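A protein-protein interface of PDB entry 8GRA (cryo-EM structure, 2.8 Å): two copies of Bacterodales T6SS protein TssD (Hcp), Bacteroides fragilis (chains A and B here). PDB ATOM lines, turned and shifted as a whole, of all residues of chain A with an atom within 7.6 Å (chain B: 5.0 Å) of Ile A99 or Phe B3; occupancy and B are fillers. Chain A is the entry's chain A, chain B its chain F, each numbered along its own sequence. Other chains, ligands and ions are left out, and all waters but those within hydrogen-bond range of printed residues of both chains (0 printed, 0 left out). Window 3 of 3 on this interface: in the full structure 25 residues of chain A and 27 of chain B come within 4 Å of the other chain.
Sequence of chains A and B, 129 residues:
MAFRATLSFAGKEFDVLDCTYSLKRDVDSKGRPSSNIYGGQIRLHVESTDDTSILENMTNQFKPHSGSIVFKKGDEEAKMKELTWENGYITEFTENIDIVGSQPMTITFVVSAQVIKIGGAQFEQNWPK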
ATOM      1  N   GLU A  47      27.057  20.848  -2.840  1.00  0.00           N
ATOM      2  CA  GLU A  47      26.581  20.469  -4.165  1.00  0.00           C
ATOM      3  C   GLU A  47      25.084  20.185  -4.113  1.00  0.00           C
ATOM      4  O   GLU A  47      24.623  19.401  -3.281  1.00  0.00           O
ATOM      5  CB  GLU A  47      27.341  19.244  -4.671  1.00  0.00           C
ATOM      6  CG  GLU A  47      26.646  18.494  -5.785  1.00  0.00           C
ATOM      7  CD  GLU A  47      26.954  19.063  -7.152  1.00  0.00           C
ATOM      8  OE1 GLU A  47      28.130  19.392  -7.407  1.00  0.00           O
ATOM      9  OE2 GLU A  47      26.023  19.174  -7.975  1.00  0.00           O
ATOM     10  N   SER A  48      24.331  20.817  -5.012  1.00  0.00           N
ATOM     11  CA  SER A  48      22.874  20.803  -4.963  1.00  0.00           C
ATOM     12  C   SER A  48      22.306  19.694  -5.837  1.00  0.00           C
ATOM     13  O   SER A  48      22.632  19.601  -7.023  1.00  0.00           O
ATOM     14  CB  SER A  48      22.316  22.150  -5.416  1.00  0.00           C
ATOM     15  OG  SER A  48      22.560  22.367  -6.792  1.00  0.00           O
ATOM     16  N   ASP A  50      18.555  18.322  -6.502  1.00  0.00           N
ATOM     17  CA  ASP A  50      17.115  18.089  -6.609  1.00  0.00           C
ATOM     18  C   ASP A  50      16.332  18.390  -5.333  1.00  0.00           C
ATOM     19  O   ASP A  50      15.114  18.192  -5.293  1.00  0.00           O
ATOM     20  CB  ASP A  50      16.857  16.637  -7.019  1.00  0.00           C
ATOM     21  CG  ASP A  50      17.416  16.311  -8.388  1.00  0.00           C
ATOM     22  OD1 ASP A  50      18.480  16.862  -8.742  1.00  0.00           O
ATOM     23  OD2 ASP A  50      16.802  15.490  -9.102  1.00  0.00           O
ATOM     24  N   ILE A  97      24.942  28.060 -11.348  1.00  0.00           N
ATOM     25  CA  ILE A  97      24.937  26.984 -12.335  1.00  0.00           C
ATOM     26  C   ILE A  97      25.833  27.392 -13.494  1.00  0.00           C
ATOM     27  O   ILE A  97      25.553  28.381 -14.176  1.00  0.00           O
ATOM     28  CB  ILE A  97      23.519  26.680 -12.843  1.00  0.00           C
ATOM     29  CG1 ILE A  97      22.574  26.446 -11.665  1.00  0.00           C
ATOM     30  CG2 ILE A  97      23.535  25.499 -13.785  1.00  0.00           C
ATOM     31  CD1 ILE A  97      21.126  26.507 -12.018  1.00  0.00           C
ATOM     32  N   ASP A  98      26.889  26.623 -13.734  1.00  0.00           N
ATOM     33  CA  ASP A  98      27.784  26.876 -14.854  1.00  0.00           C
ATOM     34  C   ASP A  98      27.848  25.633 -15.724  1.00  0.00           C
ATOM     35  O   ASP A  98      28.154  24.543 -15.232  1.00  0.00           O
ATOM     36  CB  ASP A  98      29.184  27.267 -14.381  1.00  0.00           C
ATOM     37  CG  ASP A  98      29.946  28.060 -15.423  1.00  0.00           C
ATOM     38  OD1 ASP A  98      29.606  27.952 -16.618  1.00  0.00           O
ATOM     39  OD2 ASP A  98      30.881  28.795 -15.047  1.00  0.00           O
ATOM     40  N   ILE A  99      27.571  25.801 -17.012  1.00  0.00           N
ATOM     41  CA  ILE A  99      27.474  24.685 -17.940  1.00  0.00           C
ATOM     42  C   ILE A  99      28.792  24.439 -18.663  1.00  0.00           C
ATOM     43  O   ILE A  99      29.227  23.294 -18.789  1.00  0.00           O
ATOM     44  CB  ILE A  99      26.322  24.934 -18.936  1.00  0.00           C
ATOM     45  CG1 ILE A  99      24.996  24.483 -18.325  1.00  0.00           C
ATOM     46  CG2 ILE A  99      26.575  24.228 -20.251  1.00  0.00           C
ATOM     47  CD1 ILE A  99      23.797  24.803 -19.170  1.00  0.00           C
ATOM     48  N   VAL A 100      29.442  25.505 -19.136  1.00  0.00           N
ATOM     49  CA  VAL A 100      30.722  25.354 -19.823  1.00  0.00           C
ATOM     50  C   VAL A 100      31.769  24.781 -18.876  1.00  0.00           C
ATOM     51  O   VAL A 100      32.493  23.839 -19.216  1.00  0.00           O
ATOM     52  CB  VAL A 100      31.175  26.700 -20.414  1.00  0.00           C
ATOM     53  CG1 VAL A 100      32.536  26.556 -21.076  1.00  0.00           C
ATOM     54  CG2 VAL A 100      30.144  27.226 -21.398  1.00  0.00           C
ATOM     55  N   GLY A 101      31.856  25.333 -17.669  1.00  0.00           N
ATOM     56  CA  GLY A 101      32.831  24.903 -16.691  1.00  0.00           C
ATOM     57  C   GLY A 101      32.342  23.728 -15.866  1.00  0.00           C
ATOM     58  O   GLY A 101      31.282  23.149 -16.107  1.00  0.00           O
ATOM     59  N   SER A 102      33.147  23.377 -14.866  1.00  0.00           N
ATOM     60  CA  SER A 102      32.831  22.276 -13.969  1.00  0.00           C
ATOM     61  C   SER A 102      31.891  22.769 -12.870  1.00  0.00           C
ATOM     62  O   SER A 102      31.384  23.893 -12.912  1.00  0.00           O
ATOM     63  CB  SER A 102      34.112  21.675 -13.398  1.00  0.00           C
ATOM     64  OG  SER A 102      34.722  22.565 -12.481  1.00  0.00           O
ATOM     65  N   GLN A 103      31.666  21.922 -11.858  1.00  0.00           N
ATOM     66  CA  GLN A 103      30.758  22.185 -10.747  1.00  0.00           C
ATOM     67  C   GLN A 103      29.391  22.572 -11.294  1.00  0.00           C
ATOM     68  O   GLN A 103      29.005  23.745 -11.232  1.00  0.00           O
ATOM     69  CB  GLN A 103      31.307  23.281  -9.831  1.00  0.00           C
ATOM     70  CG  GLN A 103      32.806  23.205  -9.579  1.00  0.00           C
ATOM     71  CD  GLN A 103      33.282  21.802  -9.259  1.00  0.00           C
ATOM     72  OE1 GLN A 103      34.090  21.229  -9.988  1.00  0.00           O
ATOM     73  NE2 GLN A 103      32.789  21.243  -8.160  1.00  0.00           N
ATOM     74  N   PRO A 104      28.640  21.616 -11.843  1.00  0.00           N
ATOM     75  CA  PRO A 104      27.418  21.984 -12.576  1.00  0.00           C
ATOM     76  C   PRO A 104      26.403  22.745 -11.741  1.00  0.00           C
ATOM     77  O   PRO A 104      25.749  23.660 -12.255  1.00  0.00           O
ATOM     78  CB  PRO A 104      26.877  20.624 -13.042  1.00  0.00           C
ATOM     79  CG  PRO A 104      27.422  19.643 -12.065  1.00  0.00           C
ATOM     80  CD  PRO A 104      28.779  20.161 -11.681  1.00  0.00           C
ATOM     81  N   MET A 105      26.255  22.403 -10.465  1.00  0.00           N
ATOM     82  CA  MET A 105      25.292  23.073  -9.602  1.00  0.00           C
ATOM     83  C   MET A 105      25.827  23.063  -8.181  1.00  0.00           C
ATOM     84  O   MET A 105      26.191  22.006  -7.664  1.00  0.00           O
ATOM     85  CB  MET A 105      23.925  22.389  -9.661  1.00  0.00           C
ATOM     86  CG  MET A 105      22.995  22.946 -10.714  1.00  0.00           C
ATOM     87  SD  MET A 105      21.279  22.968 -10.167  1.00  0.00           S
ATOM     88  CE  MET A 105      20.426  22.684 -11.713  1.00  0.00           C
ATOM     89  N   ALA B   2      25.710  14.748 -19.605  1.00  0.00           N
ATOM     90  CA  ALA B   2      25.952  16.166 -19.837  1.00  0.00           C
ATOM     91  C   ALA B   2      24.936  17.014 -19.083  1.00  0.00           C
ATOM     92  O   ALA B   2      24.037  16.487 -18.432  1.00  0.00           O
ATOM     93  CB  ALA B   2      25.906  16.477 -21.327  1.00  0.00           C
ATOM     94  N   PHE B   3      25.085  18.332 -19.178  1.00  0.00           N
ATOM     95  CA  PHE B   3      24.220  19.278 -18.489  1.00  0.00           C
ATOM     96  C   PHE B   3      23.781  20.350 -19.472  1.00  0.00           C
ATOM     97  O   PHE B   3      24.601  20.861 -20.240  1.00  0.00           O
ATOM     98  CB  PHE B   3      24.940  19.912 -17.298  1.00  0.00           C
ATOM     99  CG  PHE B   3      24.051  20.180 -16.125  1.00  0.00           C
ATOM    100  CD1 PHE B   3      23.095  21.176 -16.177  1.00  0.00           C
ATOM    101  CD2 PHE B   3      24.170  19.432 -14.968  1.00  0.00           C
ATOM    102  CE1 PHE B   3      22.276  21.424 -15.098  1.00  0.00           C
ATOM    103  CE2 PHE B   3      23.354  19.673 -13.885  1.00  0.00           C
ATOM    104  CZ  PHE B   3      22.405  20.671 -13.950  1.00  0.00           C
ATOM    105  N   ARG B   4      22.493  20.685 -19.451  1.00  0.00           N
ATOM    106  CA  ARG B   4      21.989  21.748 -20.305  1.00  0.00           C
ATOM    107  C   ARG B   4      20.797  22.420 -19.641  1.00  0.00           C
ATOM    108  O   ARG B   4      20.092  21.822 -18.826  1.00  0.00           O
ATOM    109  CB  ARG B   4      21.600  21.228 -21.690  1.00  0.00           C
ATOM    110  CG  ARG B   4      20.719  19.998 -21.671  1.00  0.00           C
ATOM    111  CD  ARG B   4      20.345  19.575 -23.085  1.00  0.00           C
ATOM    112  NE  ARG B   4      20.026  20.707 -23.950  1.00  0.00           N
ATOM    113  CZ  ARG B   4      19.038  21.572 -23.745  1.00  0.00           C
ATOM    114  NH1 ARG B   4      18.204  21.446 -22.725  1.00  0.00           N
ATOM    115  NH2 ARG B   4      18.879  22.585 -24.591  1.00  0.00           N
ATOM    116  N   ALA B   5      20.579  23.680 -20.013  1.00  0.00           N
ATOM    117  CA  ALA B   5      19.492  24.490 -19.488  1.00  0.00           C
ATOM    118  C   ALA B   5      18.897  25.309 -20.620  1.00  0.00           C
ATOM    119  O   ALA B   5      19.628  25.826 -21.468  1.00  0.00           O
ATOM    120  CB  ALA B   5      19.975  25.408 -18.362  1.00  0.00           C
ATOM    121  N   VAL B  16      21.151  28.426 -22.526  1.00  0.00           N
ATOM    122  CA  VAL B  16      21.774  29.069 -21.376  1.00  0.00           C
ATOM    123  C   VAL B  16      23.192  28.542 -21.213  1.00  0.00           C
ATOM    124  O   VAL B  16      23.455  27.353 -21.412  1.00  0.00           O
ATOM    125  CB  VAL B  16      20.933  28.833 -20.106  1.00  0.00           C
ATOM    126  CG1 VAL B  16      21.721  29.157 -18.858  1.00  0.00           C
ATOM    127  CG2 VAL B  16      19.666  29.657 -20.153  1.00  0.00           C
ATOM    128  N   LEU B  17      24.121  29.439 -20.873  1.00  0.00           N
ATOM    129  CA  LEU B  17      25.489  29.060 -20.560  1.00  0.00           C
ATOM    130  C   LEU B  17      25.873  29.299 -19.107  1.00  0.00           C
ATOM    131  O   LEU B  17      26.922  28.809 -18.682  1.00  0.00           O
ATOM    132  CB  LEU B  17      26.480  29.809 -21.467  1.00  0.00           C
ATOM    133  CG  LEU B  17      26.098  30.059 -22.927  1.00  0.00           C
ATOM    134  CD1 LEU B  17      26.900  31.210 -23.494  1.00  0.00           C
ATOM    135  CD2 LEU B  17      26.314  28.812 -23.754  1.00  0.00           C
ATOM    136  N   PHE B  71      16.392  23.030 -16.075  1.00  0.00           N
ATOM    137  CA  PHE B  71      17.698  22.384 -16.049  1.00  0.00           C
ATOM    138  C   PHE B  71      17.526  20.878 -16.177  1.00  0.00           C
ATOM    139  O   PHE B  71      16.661  20.291 -15.520  1.00  0.00           O
ATOM    140  CB  PHE B  71      18.453  22.723 -14.765  1.00  0.00           C
ATOM    141  CG  PHE B  71      18.268  24.138 -14.312  1.00  0.00           C
ATOM    142  CD1 PHE B  71      18.973  25.164 -14.912  1.00  0.00           C
ATOM    143  CD2 PHE B  71      17.387  24.447 -13.294  1.00  0.00           C
ATOM    144  CE1 PHE B  71      18.805  26.465 -14.504  1.00  0.00           C
ATOM    145  CE2 PHE B  71      17.217  25.751 -12.883  1.00  0.00           C
ATOM    146  CZ  PHE B  71      17.927  26.757 -13.486  1.00  0.00           C
ATOM    147  N   LYS B  72      18.349  20.256 -17.022  1.00  0.00           N
ATOM    148  CA  LYS B  72      18.245  18.829 -17.302  1.00  0.00           C
ATOM    149  C   LYS B  72      19.629  18.204 -17.395  1.00  0.00           C
ATOM    150  O   LYS B  72      20.569  18.826 -17.895  1.00  0.00           O
ATOM    151  CB  LYS B  72      17.482  18.569 -18.603  1.00  0.00           C
ATOM    152  CG  LYS B  72      16.014  18.929 -18.536  1.00  0.00           C
ATOM    153  CD  LYS B  72      15.276  18.446 -19.765  1.00  0.00           C
ATOM    154  CE  LYS B  72      15.709  19.205 -21.000  1.00  0.00           C
ATOM    155  NZ  LYS B  72      14.898  18.809 -22.182  1.00  0.00           N
ATOM    156  N   LYS B  73      19.745  16.971 -16.908  1.00  0.00           N
ATOM    157  CA  LYS B  73      20.972  16.199 -17.054  1.00  0.00           C
ATOM    158  C   LYS B  73      20.942  15.452 -18.382  1.00  0.00           C
ATOM    159  O   LYS B  73      20.057  14.621 -18.613  1.00  0.00           O
ATOM    160  CB  LYS B  73      21.136  15.222 -15.893  1.00  0.00           C
ATOM    161  CG  LYS B  73      22.153  15.651 -14.851  1.00  0.00           C
ATOM    162  CD  LYS B  73      23.575  15.432 -15.348  1.00  0.00           C
ATOM    163  CE  LYS B  73      23.769  14.024 -15.888  1.00  0.00           C
ATOM    164  NZ  LYS B  73      25.209  13.655 -15.977  1.00  0.00           N
ATOM    165  N   GLY B  74      21.910  15.740 -19.248  1.00  0.00           N
ATOM    166  CA  GLY B  74      21.950  15.145 -20.570  1.00  0.00           C
ATOM    167  C   GLY B  74      22.066  13.635 -20.560  1.00  0.00           C
ATOM    168  O   GLY B  74      22.982  13.084 -19.941  1.00  0.00           O
ATOM    169  N   MET B  80      14.909  18.014 -13.596  1.00  0.00           N
ATOM    170  CA  MET B  80      15.002  17.965 -12.144  1.00  0.00           C
ATOM    171  C   MET B  80      14.619  19.258 -11.443  1.00  0.00           C
ATOM    172  O   MET B  80      14.188  19.197 -10.286  1.00  0.00           O
ATOM    173  CB  MET B  80      16.426  17.592 -11.713  1.00  0.00           C
ATOM    174  CG  MET B  80      17.445  18.667 -12.019  1.00  0.00           C
ATOM    175  SD  MET B  80      19.140  18.099 -11.872  1.00  0.00           S
ATOM    176  CE  MET B  80      19.397  17.476 -13.527  1.00  0.00           C
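The side-chain carboxylate (OD1) of Asp A50 sits close to the side-chain sulfur (SD) of Met B80 (3.4 Å). The side-chain carboxylate (OD1) of Asp A98 sits close to the backbone carbonyl oxygen (O) of Leu B17 (3.5 Å).
Glu A47 touches none of the printed residues of chain B. Of the printed residues of chain B, Asp A50 touches Met B80. Printed residues of chain B within 4 Å of Ile A97: Phe B71. Of the printed residues of chain B, Asp A98 touches Leu B17 (3.5 Å). Ile A99 touches just these residues of chain B: Phe B3, Arg B4, Ala B5, Val B16 and Leu B17. Of chain A, only Ile A99, Pro A104 and Met A105 come within 4 Å of Phe B3. Of the printed residues of chain A, Ala B5 touches Ile A99 (3.5 Å). Of the printed residues of chain A, Val B16 touches Ile A99 (3.4 Å). The nearest printed residue of chain B that does not touch Ile A99 is Phe B71 (6.4 Å).
N of Ser A48 lies within hydrogen-bond range of O of Met A105. O of Arg B4 lies within hydrogen-bond range of N of Lys B72 (3.0 Å). N of Val B16 is in hydrogen-bond range of O of Ala B5 (3.2 Å). The backbone NH (N) of Met B80 is in hydrogen-bond range of the backbone carbonyl oxygen (O) of Phe B71.
Of the 11 printed residues of chain B, 7 touch a printed residue of chain A. Among the printed residues, no Asp or Glu carboxylate lies within 4 Å of a Lys or Arg side-chain nitrogen of the other chain.
Among the printed residues, merely in contact across the chains: Ile A97 with Phe B71 (3.4 Å), Ile A99 with Val B16 (3.4 Å), Ile A99 with Leu B17 (3.5 Å), Ile A99 with Ala B5 (3.5 Å), Pro A104 with Phe B3 (3.5 Å), Met A105 with Phe B3 (3.6 Å), Met A105 with Phe B71 (3.6 Å), Ile A99 with Arg B4 (3.7 Å) and Ile A99 with Phe B3 (3.9 Å).
No position is printed for both chains.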
